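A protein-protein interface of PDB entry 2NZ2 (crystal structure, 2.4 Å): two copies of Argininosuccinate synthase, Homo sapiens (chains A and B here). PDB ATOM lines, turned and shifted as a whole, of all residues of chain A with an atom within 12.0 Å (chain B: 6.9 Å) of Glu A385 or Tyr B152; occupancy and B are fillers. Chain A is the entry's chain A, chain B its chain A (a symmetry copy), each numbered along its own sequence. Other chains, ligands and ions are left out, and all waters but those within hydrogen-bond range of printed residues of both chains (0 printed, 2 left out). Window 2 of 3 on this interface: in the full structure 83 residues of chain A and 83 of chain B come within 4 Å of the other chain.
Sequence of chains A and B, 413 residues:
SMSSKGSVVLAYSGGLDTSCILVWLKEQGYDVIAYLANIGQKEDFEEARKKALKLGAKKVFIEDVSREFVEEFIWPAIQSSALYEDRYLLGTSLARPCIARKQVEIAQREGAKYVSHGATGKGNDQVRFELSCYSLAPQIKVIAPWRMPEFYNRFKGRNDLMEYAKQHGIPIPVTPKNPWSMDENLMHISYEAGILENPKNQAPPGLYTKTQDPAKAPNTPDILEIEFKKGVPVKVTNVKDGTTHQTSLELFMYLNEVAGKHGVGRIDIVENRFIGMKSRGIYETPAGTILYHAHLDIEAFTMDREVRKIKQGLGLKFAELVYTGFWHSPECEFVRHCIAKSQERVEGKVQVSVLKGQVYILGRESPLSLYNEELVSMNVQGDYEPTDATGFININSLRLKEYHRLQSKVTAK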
ATOM      1  N   ASN A 372     -18.399 -10.532  46.258  1.00  0.00           N
ATOM      2  CA  ASN A 372     -18.209 -11.500  45.179  1.00  0.00           C
ATOM      3  C   ASN A 372     -16.922 -11.172  44.440  1.00  0.00           C
ATOM      4  O   ASN A 372     -16.881 -10.326  43.573  1.00  0.00           O
ATOM      5  CB  ASN A 372     -19.408 -11.525  44.222  1.00  0.00           C
ATOM      6  CG  ASN A 372     -19.335 -12.659  43.198  1.00  0.00           C
ATOM      7  OD1 ASN A 372     -18.267 -13.149  42.857  1.00  0.00           O
ATOM      8  ND2 ASN A 372     -20.487 -13.070  42.707  1.00  0.00           N
ATOM      9  N   GLU A 374     -15.307 -12.928  42.296  1.00  0.00           N
ATOM     10  CA  GLU A 374     -15.345 -13.337  40.884  1.00  0.00           C
ATOM     11  C   GLU A 374     -16.024 -12.317  39.984  1.00  0.00           C
ATOM     12  O   GLU A 374     -15.545 -12.025  38.876  1.00  0.00           O
ATOM     13  CB  GLU A 374     -16.053 -14.691  40.731  1.00  0.00           C
ATOM     14  CG  GLU A 374     -15.315 -15.678  39.836  1.00  0.00           C
ATOM     15  CD  GLU A 374     -16.232 -16.391  38.847  1.00  0.00           C
ATOM     16  OE1 GLU A 374     -15.960 -16.276  37.617  1.00  0.00           O
ATOM     17  OE2 GLU A 374     -17.212 -17.047  39.299  1.00  0.00           O
ATOM     18  N   LEU A 375     -17.146 -11.794  40.469  1.00  0.00           N
ATOM     19  CA  LEU A 375     -17.963 -10.798  39.778  1.00  0.00           C
ATOM     20  C   LEU A 375     -17.266  -9.457  39.612  1.00  0.00           C
ATOM     21  O   LEU A 375     -17.328  -8.861  38.541  1.00  0.00           O
ATOM     22  CB  LEU A 375     -19.279 -10.597  40.542  1.00  0.00           C
ATOM     23  CG  LEU A 375     -20.332  -9.632  39.999  1.00  0.00           C
ATOM     24  CD1 LEU A 375     -20.992 -10.161  38.732  1.00  0.00           C
ATOM     25  CD2 LEU A 375     -21.358  -9.312  41.067  1.00  0.00           C
ATOM     26  N   VAL A 376     -16.619  -8.975  40.667  1.00  0.00           N
ATOM     27  CA  VAL A 376     -15.921  -7.675  40.629  1.00  0.00           C
ATOM     28  C   VAL A 376     -14.574  -7.731  39.873  1.00  0.00           C
ATOM     29  O   VAL A 376     -13.984  -6.705  39.558  1.00  0.00           O
ATOM     30  CB  VAL A 376     -15.739  -7.090  42.072  1.00  0.00           C
ATOM     31  CG1 VAL A 376     -14.384  -7.498  42.677  1.00  0.00           C
ATOM     32  CG2 VAL A 376     -15.913  -5.561  42.072  1.00  0.00           C
ATOM     33  N   SER A 377     -14.104  -8.940  39.579  1.00  0.00           N
ATOM     34  CA  SER A 377     -12.821  -9.157  38.933  1.00  0.00           C
ATOM     35  C   SER A 377     -12.552  -8.195  37.782  1.00  0.00           C
ATOM     36  O   SER A 377     -13.192  -8.283  36.739  1.00  0.00           O
ATOM     37  CB  SER A 377     -12.718 -10.594  38.430  1.00  0.00           C
ATOM     38  OG  SER A 377     -11.531 -10.743  37.683  1.00  0.00           O
ATOM     39  N   ASN A 379     -10.509  -8.644  35.126  1.00  0.00           N
ATOM     40  CA  ASN A 379      -9.571  -9.473  34.379  1.00  0.00           C
ATOM     41  C   ASN A 379     -10.231 -10.732  33.824  1.00  0.00           C
ATOM     42  O   ASN A 379      -9.727 -11.369  32.912  1.00  0.00           O
ATOM     43  CB  ASN A 379      -8.373  -9.850  35.252  1.00  0.00           C
ATOM     44  N   VAL A 380     -11.394 -11.074  34.395  1.00  0.00           N
ATOM     45  CA  VAL A 380     -12.137 -12.252  33.963  1.00  0.00           C
ATOM     46  C   VAL A 380     -13.640 -11.991  33.979  1.00  0.00           C
ATOM     47  O   VAL A 380     -14.364 -12.527  34.818  1.00  0.00           O
ATOM     48  CB  VAL A 380     -11.828 -13.471  34.851  1.00  0.00           C
ATOM     49  N   GLN A 381     -14.007 -11.380  33.233  1.00  0.00           N
ATOM     50  CA  GLN A 381     -15.370 -11.562  32.748  1.00  0.00           C
ATOM     51  C   GLN A 381     -16.353 -11.694  33.905  1.00  0.00           C
ATOM     52  O   GLN A 381     -16.919 -10.703  34.368  1.00  0.00           O
ATOM     53  CB  GLN A 381     -15.455 -12.791  31.840  1.00  0.00           C
ATOM     54  N   GLY A 382     -16.821 -12.751  33.682  1.00  0.00           N
ATOM     55  CA  GLY A 382     -17.640 -13.530  34.592  1.00  0.00           C
ATOM     56  C   GLY A 382     -19.121 -13.258  34.415  1.00  0.00           C
ATOM     57  O   GLY A 382     -19.563 -12.871  33.312  1.00  0.00           O
ATOM     58  N   ASP A 383     -19.900 -13.426  35.468  1.00  0.00           N
ATOM     59  CA  ASP A 383     -21.338 -13.191  35.420  1.00  0.00           C
ATOM     60  C   ASP A 383     -21.651 -11.702  35.332  1.00  0.00           C
ATOM     61  O   ASP A 383     -22.012 -11.073  36.327  1.00  0.00           O
ATOM     62  CB  ASP A 383     -22.021 -13.800  36.646  1.00  0.00           C
ATOM     63  CG  ASP A 383     -23.482 -13.409  36.753  1.00  0.00           C
ATOM     64  OD1 ASP A 383     -24.115 -13.176  35.702  1.00  0.00           O
ATOM     65  OD2 ASP A 383     -23.998 -13.334  37.887  1.00  0.00           O
ATOM     66  N   TYR A 384     -21.508 -11.142  34.135  1.00  0.00           N
ATOM     67  CA  TYR A 384     -21.768  -9.762  33.920  1.00  0.00           C
ATOM     68  C   TYR A 384     -21.892  -9.479  32.435  1.00  0.00           C
ATOM     69  O   TYR A 384     -21.298 -10.094  31.629  1.00  0.00           O
ATOM     70  CB  TYR A 384     -20.722  -8.900  34.628  1.00  0.00           C
ATOM     71  CG  TYR A 384     -20.926  -7.430  34.558  1.00  0.00           C
ATOM     72  CD1 TYR A 384     -21.859  -6.817  35.315  1.00  0.00           C
ATOM     73  CD2 TYR A 384     -20.162  -6.658  33.760  1.00  0.00           C
ATOM     74  CE1 TYR A 384     -22.040  -5.522  35.266  1.00  0.00           C
ATOM     75  CE2 TYR A 384     -20.344  -5.343  33.725  1.00  0.00           C
ATOM     76  CZ  TYR A 384     -21.284  -4.779  34.491  1.00  0.00           C
ATOM     77  OH  TYR A 384     -21.492  -3.464  34.477  1.00  0.00           O
ATOM     78  N   GLU A 385     -22.724  -8.542  32.099  1.00  0.00           N
ATOM     79  CA  GLU A 385     -22.829  -8.083  30.760  1.00  0.00           C
ATOM     80  C   GLU A 385     -22.484  -6.612  30.645  1.00  0.00           C
ATOM     81  O   GLU A 385     -23.213  -5.798  31.069  1.00  0.00           O
ATOM     82  CB  GLU A 385     -24.188  -8.437  30.193  1.00  0.00           C
ATOM     83  CG  GLU A 385     -24.461  -7.962  28.823  1.00  0.00           C
ATOM     84  CD  GLU A 385     -23.427  -8.355  27.832  1.00  0.00           C
ATOM     85  OE1 GLU A 385     -22.903  -7.448  27.235  1.00  0.00           O
ATOM     86  OE2 GLU A 385     -23.166  -9.551  27.672  1.00  0.00           O
ATOM     87  N   PRO A 386     -21.309  -6.299  30.125  1.00  0.00           N
ATOM     88  CA  PRO A 386     -20.854  -4.903  30.045  1.00  0.00           C
ATOM     89  C   PRO A 386     -21.796  -3.979  29.269  1.00  0.00           C
ATOM     90  O   PRO A 386     -21.833  -2.788  29.514  1.00  0.00           O
ATOM     91  CB  PRO A 386     -19.505  -5.005  29.316  1.00  0.00           C
ATOM     92  CG  PRO A 386     -19.059  -6.431  29.492  1.00  0.00           C
ATOM     93  CD  PRO A 386     -20.285  -7.258  29.662  1.00  0.00           C
ATOM     94  N   THR A 387     -22.528  -4.544  28.325  1.00  0.00           N
ATOM     95  CA  THR A 387     -23.565  -3.860  27.551  1.00  0.00           C
ATOM     96  C   THR A 387     -24.740  -3.321  28.407  1.00  0.00           C
ATOM     97  O   THR A 387     -25.454  -2.405  27.998  1.00  0.00           O
ATOM     98  CB  THR A 387     -23.996  -4.799  26.390  1.00  0.00           C
ATOM     99  OG1 THR A 387     -23.271  -4.427  25.199  1.00  0.00           O
ATOM    100  CG2 THR A 387     -25.494  -4.779  26.121  1.00  0.00           C
ATOM    101  N   ASP A 388     -24.995  -3.885  29.577  1.00  0.00           N
ATOM    102  CA  ASP A 388     -26.024  -3.458  30.502  1.00  0.00           C
ATOM    103  C   ASP A 388     -26.019  -2.050  31.118  1.00  0.00           C
ATOM    104  O   ASP A 388     -26.916  -1.351  30.951  1.00  0.00           O
ATOM    105  CB  ASP A 388     -26.319  -4.517  31.568  1.00  0.00           C
ATOM    106  CG  ASP A 388     -26.977  -5.737  31.024  1.00  0.00           C
ATOM    107  OD1 ASP A 388     -27.800  -5.643  30.152  1.00  0.00           O
ATOM    108  OD2 ASP A 388     -26.660  -6.787  31.459  1.00  0.00           O
ATOM    109  N   ALA A 389     -24.778  -1.758  31.491  1.00  0.00           N
ATOM    110  CA  ALA A 389     -24.185  -0.609  32.066  1.00  0.00           C
ATOM    111  C   ALA A 389     -24.275   0.546  31.160  1.00  0.00           C
ATOM    112  O   ALA A 389     -24.485   1.606  31.603  1.00  0.00           O
ATOM    113  CB  ALA A 389     -22.844  -0.895  32.350  1.00  0.00           C
ATOM    114  N   THR A 390     -24.150   0.292  29.870  1.00  0.00           N
ATOM    115  CA  THR A 390     -24.382   1.258  28.875  1.00  0.00           C
ATOM    116  C   THR A 390     -25.830   1.745  28.925  1.00  0.00           C
ATOM    117  O   THR A 390     -26.056   2.898  28.985  1.00  0.00           O
ATOM    118  CB  THR A 390     -23.710   1.050  27.500  1.00  0.00           C
ATOM    119  OG1 THR A 390     -24.575   1.379  26.450  1.00  0.00           O
ATOM    120  CG2 THR A 390     -23.193  -0.163  27.300  1.00  0.00           C
ATOM    121  N   GLY A 391     -26.781   0.851  29.046  1.00  0.00           N
ATOM    122  CA  GLY A 391     -28.173   1.201  29.234  1.00  0.00           C
ATOM    123  C   GLY A 391     -28.487   1.945  30.534  1.00  0.00           C
ATOM    124  O   GLY A 391     -29.243   2.854  30.535  1.00  0.00           O
ATOM    125  N   PHE A 392     -27.874   1.481  31.609  1.00  0.00           N
ATOM    126  CA  PHE A 392     -27.894   2.060  32.956  1.00  0.00           C
ATOM    127  C   PHE A 392     -27.376   3.488  32.984  1.00  0.00           C
ATOM    128  O   PHE A 392     -27.964   4.349  33.628  1.00  0.00           O
ATOM    129  CB  PHE A 392     -27.069   1.149  33.888  1.00  0.00           C
ATOM    130  CG  PHE A 392     -26.925   1.647  35.303  1.00  0.00           C
ATOM    131  CD1 PHE A 392     -27.957   1.483  36.231  1.00  0.00           C
ATOM    132  CD2 PHE A 392     -25.719   2.228  35.735  1.00  0.00           C
ATOM    133  CE1 PHE A 392     -27.816   1.920  37.545  1.00  0.00           C
ATOM    134  CE2 PHE A 392     -25.571   2.663  37.036  1.00  0.00           C
ATOM    135  CZ  PHE A 392     -26.632   2.514  37.947  1.00  0.00           C
ATOM    136  N   ILE A 393     -26.261   3.744  32.308  1.00  0.00           N
ATOM    137  CA  ILE A 393     -25.721   5.101  32.205  1.00  0.00           C
ATOM    138  C   ILE A 393     -26.678   5.961  31.394  1.00  0.00           C
ATOM    139  O   ILE A 393     -27.044   7.040  31.821  1.00  0.00           O
ATOM    140  CB  ILE A 393     -24.291   5.123  31.578  1.00  0.00           C
ATOM    141  CG1 ILE A 393     -23.247   4.777  32.641  1.00  0.00           C
ATOM    142  CG2 ILE A 393     -23.969   6.497  30.987  1.00  0.00           C
ATOM    143  CD1 ILE A 393     -21.897   4.416  32.092  1.00  0.00           C
ATOM    144  N   ASN A 394     -27.084   5.449  30.234  1.00  0.00           N
ATOM    145  CA  ASN A 394     -27.873   6.199  29.273  1.00  0.00           C
ATOM    146  C   ASN A 394     -29.240   6.607  29.770  1.00  0.00           C
ATOM    147  O   ASN A 394     -29.750   7.660  29.401  1.00  0.00           O
ATOM    148  CB  ASN A 394     -27.999   5.428  27.965  1.00  0.00           C
ATOM    149  CG  ASN A 394     -26.728   5.483  27.138  1.00  0.00           C
ATOM    150  OD1 ASN A 394     -25.837   6.277  27.411  1.00  0.00           O
ATOM    151  ND2 ASN A 394     -26.636   4.630  26.133  1.00  0.00           N
ATOM    152  N   TRP B  24      -6.577   1.753  18.710  1.00  0.00           N
ATOM    153  CA  TRP B  24      -7.820   1.071  18.297  1.00  0.00           C
ATOM    154  C   TRP B  24      -8.847   2.001  17.629  1.00  0.00           C
ATOM    155  O   TRP B  24      -9.362   1.670  16.575  1.00  0.00           O
ATOM    156  CB  TRP B  24      -8.437   0.319  19.484  1.00  0.00           C
ATOM    157  CG  TRP B  24      -9.651  -0.536  19.138  1.00  0.00           C
ATOM    158  CD1 TRP B  24      -9.646  -1.821  18.655  1.00  0.00           C
ATOM    159  CD2 TRP B  24     -11.029  -0.183  19.298  1.00  0.00           C
ATOM    160  NE1 TRP B  24     -10.918  -2.268  18.484  1.00  0.00           N
ATOM    161  CE2 TRP B  24     -11.793  -1.291  18.871  1.00  0.00           C
ATOM    162  CE3 TRP B  24     -11.694   0.963  19.760  1.00  0.00           C
ATOM    163  CZ2 TRP B  24     -13.187  -1.283  18.885  1.00  0.00           C
ATOM    164  CZ3 TRP B  24     -13.080   0.977  19.772  1.00  0.00           C
ATOM    165  CH2 TRP B  24     -13.810  -0.130  19.341  1.00  0.00           C
ATOM    166  N   GLY B 121     -16.045  -1.758  32.463  1.00  0.00           N
ATOM    167  CA  GLY B 121     -17.497  -1.947  32.402  1.00  0.00           C
ATOM    168  C   GLY B 121     -18.161  -2.187  33.745  1.00  0.00           C
ATOM    169  O   GLY B 121     -19.383  -2.145  33.853  1.00  0.00           O
ATOM    170  N   LYS B 122     -17.346  -2.411  34.771  1.00  0.00           N
ATOM    171  CA  LYS B 122     -17.803  -2.743  36.109  1.00  0.00           C
ATOM    172  C   LYS B 122     -17.501  -1.621  37.111  1.00  0.00           C
ATOM    173  O   LYS B 122     -17.765  -1.768  38.311  1.00  0.00           O
ATOM    174  CB  LYS B 122     -17.094  -4.007  36.575  1.00  0.00           C
ATOM    175  CG  LYS B 122     -17.285  -5.215  35.660  1.00  0.00           C
ATOM    176  CD  LYS B 122     -16.334  -6.347  36.026  1.00  0.00           C
ATOM    177  CE  LYS B 122     -16.923  -7.696  35.628  1.00  0.00           C
ATOM    178  NZ  LYS B 122     -16.102  -8.824  36.168  1.00  0.00           N
ATOM    179  N   ALA B 144     -17.071   3.982  24.595  1.00  0.00           N
ATOM    180  CA  ALA B 144     -16.518   3.318  25.773  1.00  0.00           C
ATOM    181  C   ALA B 144     -16.173   1.869  25.366  1.00  0.00           C
ATOM    182  O   ALA B 144     -17.006   0.951  25.542  1.00  0.00           O
ATOM    183  CB  ALA B 144     -17.529   3.344  26.902  1.00  0.00           C
ATOM    184  N   PRO B 145     -14.966   1.672  24.784  1.00  0.00           N
ATOM    185  CA  PRO B 145     -14.513   0.387  24.219  1.00  0.00           C
ATOM    186  C   PRO B 145     -14.769  -0.831  25.139  1.00  0.00           C
ATOM    187  O   PRO B 145     -15.279  -1.873  24.678  1.00  0.00           O
ATOM    188  CB  PRO B 145     -13.004   0.611  24.014  1.00  0.00           C
ATOM    189  CG  PRO B 145     -12.866   2.076  23.796  1.00  0.00           C
ATOM    190  CD  PRO B 145     -13.944   2.729  24.614  1.00  0.00           C
ATOM    191  N   TRP B 146     -14.446  -0.692  26.423  1.00  0.00           N
ATOM    192  CA  TRP B 146     -14.729  -1.742  27.410  1.00  0.00           C
ATOM    193  C   TRP B 146     -16.212  -2.206  27.493  1.00  0.00           C
ATOM    194  O   TRP B 146     -16.501  -3.229  28.101  1.00  0.00           O
ATOM    195  CB  TRP B 146     -14.164  -1.367  28.785  1.00  0.00           C
ATOM    196  CG  TRP B 146     -12.663  -1.447  28.850  1.00  0.00           C
ATOM    197  CD1 TRP B 146     -11.786  -0.429  29.188  1.00  0.00           C
ATOM    198  CD2 TRP B 146     -11.841  -2.604  28.594  1.00  0.00           C
ATOM    199  NE1 TRP B 146     -10.482  -0.883  29.153  1.00  0.00           N
ATOM    200  CE2 TRP B 146     -10.480  -2.208  28.791  1.00  0.00           C
ATOM    201  CE3 TRP B 146     -12.111  -3.939  28.212  1.00  0.00           C
ATOM    202  CZ2 TRP B 146      -9.399  -3.103  28.614  1.00  0.00           C
ATOM    203  CZ3 TRP B 146     -11.026  -4.825  28.043  1.00  0.00           C
ATOM    204  CH2 TRP B 146      -9.695  -4.403  28.246  1.00  0.00           C
ATOM    205  N   ARG B 147     -17.119  -1.472  26.842  1.00  0.00           N
ATOM    206  CA  ARG B 147     -18.535  -1.859  26.730  1.00  0.00           C
ATOM    207  C   ARG B 147     -18.915  -2.239  25.303  1.00  0.00           C
ATOM    208  O   ARG B 147     -20.075  -2.622  25.030  1.00  0.00           O
ATOM    209  CB  ARG B 147     -19.462  -0.751  27.256  1.00  0.00           C
ATOM    210  CG  ARG B 147     -19.205  -0.394  28.735  1.00  0.00           C
ATOM    211  CD  ARG B 147     -20.428   0.213  29.370  1.00  0.00           C
ATOM    212  NE  ARG B 147     -20.966   1.321  28.581  1.00  0.00           N
ATOM    213  CZ  ARG B 147     -20.661   2.590  28.790  1.00  0.00           C
ATOM    214  NH1 ARG B 147     -21.192   3.539  28.029  1.00  0.00           N
ATOM    215  NH2 ARG B 147     -19.824   2.906  29.764  1.00  0.00           N
ATOM    216  N   MET B 148     -17.940  -2.133  24.401  1.00  0.00           N
ATOM    217  CA  MET B 148     -18.121  -2.600  23.029  1.00  0.00           C
ATOM    218  C   MET B 148     -17.697  -4.062  22.872  1.00  0.00           C
ATOM    219  O   MET B 148     -16.558  -4.414  23.160  1.00  0.00           O
ATOM    220  CB  MET B 148     -17.395  -1.673  22.045  1.00  0.00           C
ATOM    221  CG  MET B 148     -18.062  -0.309  22.002  1.00  0.00           C
ATOM    222  SD  MET B 148     -17.044   1.015  21.369  1.00  0.00           S
ATOM    223  CE  MET B 148     -17.247   0.772  19.597  1.00  0.00           C
ATOM    224  N   PRO B 149     -18.636  -4.935  22.477  1.00  0.00           N
ATOM    225  CA  PRO B 149     -18.304  -6.346  22.192  1.00  0.00           C
ATOM    226  C   PRO B 149     -17.085  -6.544  21.264  1.00  0.00           C
ATOM    227  O   PRO B 149     -16.152  -7.271  21.616  1.00  0.00           O
ATOM    228  CB  PRO B 149     -19.596  -6.884  21.557  1.00  0.00           C
ATOM    229  CG  PRO B 149     -20.684  -6.044  22.175  1.00  0.00           C
ATOM    230  CD  PRO B 149     -20.082  -4.665  22.330  1.00  0.00           C
ATOM    231  N   GLU B 150     -17.069  -5.884  20.108  1.00  0.00           N
ATOM    232  CA  GLU B 150     -15.917  -5.982  19.194  1.00  0.00           C
ATOM    233  C   GLU B 150     -14.553  -5.789  19.913  1.00  0.00           C
ATOM    234  O   GLU B 150     -13.543  -6.367  19.504  1.00  0.00           O
ATOM    235  CB  GLU B 150     -16.072  -5.048  17.980  1.00  0.00           C
ATOM    236  CG  GLU B 150     -16.353  -3.556  18.322  1.00  0.00           C
ATOM    237  CD  GLU B 150     -17.848  -3.177  18.329  1.00  0.00           C
ATOM    238  OE1 GLU B 150     -18.652  -3.686  19.177  1.00  0.00           O
ATOM    239  OE2 GLU B 150     -18.202  -2.329  17.482  1.00  0.00           O
ATOM    240  N   PHE B 151     -14.556  -5.014  21.001  1.00  0.00           N
ATOM    241  CA  PHE B 151     -13.354  -4.671  21.763  1.00  0.00           C
ATOM    242  C   PHE B 151     -13.173  -5.588  22.991  1.00  0.00           C
ATOM    243  O   PHE B 151     -12.127  -6.205  23.146  1.00  0.00           O
ATOM    244  CB  PHE B 151     -13.411  -3.176  22.183  1.00  0.00           C
ATOM    245  CG  PHE B 151     -12.150  -2.659  22.848  1.00  0.00           C
ATOM    246  CD1 PHE B 151     -11.931  -2.836  24.208  1.00  0.00           C
ATOM    247  CD2 PHE B 151     -11.185  -1.972  22.109  1.00  0.00           C
ATOM    248  CE1 PHE B 151     -10.760  -2.359  24.822  1.00  0.00           C
ATOM    249  CE2 PHE B 151     -10.009  -1.491  22.719  1.00  0.00           C
ATOM    250  CZ  PHE B 151      -9.818  -1.689  24.085  1.00  0.00           C
ATOM    251  N   TYR B 152     -14.183  -5.692  23.853  1.00  0.00           N
ATOM    252  CA  TYR B 152     -13.982  -6.375  25.139  1.00  0.00           C
ATOM    253  C   TYR B 152     -13.906  -7.906  25.077  1.00  0.00           C
ATOM    254  O   TYR B 152     -13.272  -8.530  25.929  1.00  0.00           O
ATOM    255  CB  TYR B 152     -14.947  -5.878  26.227  1.00  0.00           C
ATOM    256  CG  TYR B 152     -16.386  -6.322  26.107  1.00  0.00           C
ATOM    257  CD1 TYR B 152     -17.402  -5.395  25.983  1.00  0.00           C
ATOM    258  CD2 TYR B 152     -16.729  -7.674  26.160  1.00  0.00           C
ATOM    259  CE1 TYR B 152     -18.742  -5.795  25.886  1.00  0.00           C
ATOM    260  CE2 TYR B 152     -18.040  -8.085  26.049  1.00  0.00           C
ATOM    261  CZ  TYR B 152     -19.049  -7.147  25.922  1.00  0.00           C
ATOM    262  OH  TYR B 152     -20.349  -7.576  25.832  1.00  0.00           O
ATOM    263  N   ASN B 153     -14.534  -8.500  24.068  1.00  0.00           N
ATOM    264  CA  ASN B 153     -14.406  -9.933  23.800  1.00  0.00           C
ATOM    265  C   ASN B 153     -13.050 -10.298  23.161  1.00  0.00           C
ATOM    266  O   ASN B 153     -12.547 -11.404  23.384  1.00  0.00           O
ATOM    267  CB  ASN B 153     -15.584 -10.434  22.947  1.00  0.00           C
ATOM    268  CG  ASN B 153     -16.882 -10.547  23.745  1.00  0.00           C
ATOM    269  OD1 ASN B 153     -16.888 -10.984  24.905  1.00  0.00           O
ATOM    270  ND2 ASN B 153     -17.990 -10.173  23.120  1.00  0.00           N
ATOM    271  N   ARG B 154     -12.410  -9.365  22.464  1.00  0.00           N
ATOM    272  CA  ARG B 154     -11.066  -9.561  21.970  1.00  0.00           C
ATOM    273  C   ARG B 154      -9.965  -9.427  23.048  1.00  0.00           C
ATOM    274  O   ARG B 154      -9.061 -10.171  23.076  1.00  0.00           O
ATOM    275  CB  ARG B 154     -10.792  -8.853  20.660  1.00  0.00           C
ATOM    276  CG  ARG B 154     -10.326  -7.474  20.714  1.00  0.00           C
ATOM    277  CD  ARG B 154     -10.194  -6.904  19.368  1.00  0.00           C
ATOM    278  NE  ARG B 154      -8.939  -7.236  18.770  1.00  0.00           N
ATOM    279  CZ  ARG B 154      -8.297  -6.481  17.911  1.00  0.00           C
ATOM    280  NH1 ARG B 154      -8.809  -5.367  17.515  1.00  0.00           N
ATOM    281  NH2 ARG B 154      -7.139  -6.858  17.427  1.00  0.00           N
ATOM    282  N   PHE B 155     -10.117  -8.522  23.982  1.00  0.00           N
ATOM    283  CA  PHE B 155      -9.161  -8.363  25.038  1.00  0.00           C
ATOM    284  C   PHE B 155      -9.798  -8.745  26.300  1.00  0.00           C
ATOM    285  O   PHE B 155     -10.165  -7.960  27.104  1.00  0.00           O
ATOM    286  CB  PHE B 155      -8.525  -6.996  25.151  1.00  0.00           C
ATOM    287  CG  PHE B 155      -8.277  -6.338  23.861  1.00  0.00           C
ATOM    288  CD1 PHE B 155      -7.301  -6.764  23.035  1.00  0.00           C
ATOM    289  CD2 PHE B 155      -9.039  -5.304  23.475  1.00  0.00           C
ATOM    290  CE1 PHE B 155      -7.125  -6.170  21.891  1.00  0.00           C
ATOM    291  CE2 PHE B 155      -8.840  -4.729  22.336  1.00  0.00           C
ATOM    292  CZ  PHE B 155      -7.890  -5.136  21.546  1.00  0.00           C
ATOM    293  N   LYS B 156      -9.903 -10.040  26.390  1.00  0.00           N
ATOM    294  CA  LYS B 156     -10.463 -10.788  27.423  1.00  0.00           C
ATOM    295  C   LYS B 156      -9.608 -10.678  28.647  1.00  0.00           C
ATOM    296  O   LYS B 156     -10.103 -10.551  29.734  1.00  0.00           O
ATOM    297  CB  LYS B 156     -10.471 -12.218  26.927  1.00  0.00           C
ATOM    298  CG  LYS B 156      -9.225 -13.015  27.357  1.00  0.00           C
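O of Leu A375 lies within hydrogen-bond range of NZ of Lys B122.
The side-chain amino group of Lys B122 is in hydrogen-bond range of the backbone carbonyl oxygen of Ser A377, at 3.0 Å.
The side-chain amino group (NZ) of Lys B122 lies within hydrogen-bond range of the backbone carbonyl oxygen (O) of Gln A381, at 2.7 Å.
The backbone carbonyl oxygen (O) of Gly B121 sits at hydrogen-bond distance from the side-chain hydroxyl (OH) of Tyr A384 (2.6 Å).
OE1 of Glu A385 is in hydrogen-bond range of OH of Tyr B152.
O of Asn A379 sits close to O of Lys B156, 3.3 Å away.
CG of Lys B122 touches CE2 of Tyr A384, at 3.6 Å.
Pro A386 touches Trp B146 (CB to O, 3.7 Å).
Arg B147 touches Pro A386.
CB of Pro A386 touches CE1 of Tyr B152 (3.6 Å).
Thr A387 touches Arg B147.
CB of Ala A389 touches O of Gly B121, 3.97 Å away.
Ala A389 touches Arg B147 (CB to CD, 3.99 Å).
Arg B147 touches Thr A390 (NE to CB, 3.0 Å).
Ile A393 touches Arg B147 (CD1 to NH2, 3.5 Å).
Hydrophobic or aromatic side chains of chain A within 4 Å of the printed part of chain B: Tyr A384, Pro A386, Ala A389 and Ile A393.
Of the 16 printed residues of chain B, 6 touch a printed residue of chain A.
Along chain B the printed residues that touch a printed residue of chain A span positions 121 to 156.
Among the printed residues, 15 pairs touch across the chains.
Among the printed residues, no Asp or Glu carboxylate lies within 4 Å of a Lys or Arg side-chain nitrogen of the other chain.
The backbone NH (N) of Leu A375 is in hydrogen-bond range of the side-chain amide oxygen (OD1) of Asn A372 (3.0 Å).
The backbone NH (N) of Asn A379 sits close to the side-chain hydroxyl (OG) of Ser A377 (3.5 Å).
The side-chain hydroxyl (OG) of Ser A377 lies within hydrogen-bond range of the backbone NH (N) of Val A380, at 3.3 Å.
The side-chain carboxylate (OE1) of Glu A385 lies close to the backbone NH (N) of Thr A387, 3.1 Å away.
The side-chain amide nitrogen (ND2) of Asn A394 sits close to the backbone carbonyl oxygen (O) of Thr A390 (3.4 Å).
No position is printed for both chains.
Glu A385 touches just one residue of chain B: Tyr B152.
Gly B121 touches just these residues of chain A: Tyr A384 and Ala A389.
No residue of chain A comes within 4 Å of Pro B149.
No residue of chain A comes within 4 Å of Asn B153.
Printed residues of chain B within 4 Å of Thr A387: Arg B147.
Of the printed residues of chain B, Thr A390 touches Arg B147.
Printed residues of chain B within 4 Å of Ser A377: Lys B122.
Of the printed residues of chain B, Ile A393 touches Arg B147.
Printed residues of chain B within 4 Å of Tyr A384: Gly B121 and Lys B122.
Glu B150 touches none of the printed residues of chain A.
Arg B154 touches none of the printed residues of chain A.
The nearest residue of chain A that does not touch Tyr B152 is Thr A387 (4.3 Å).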
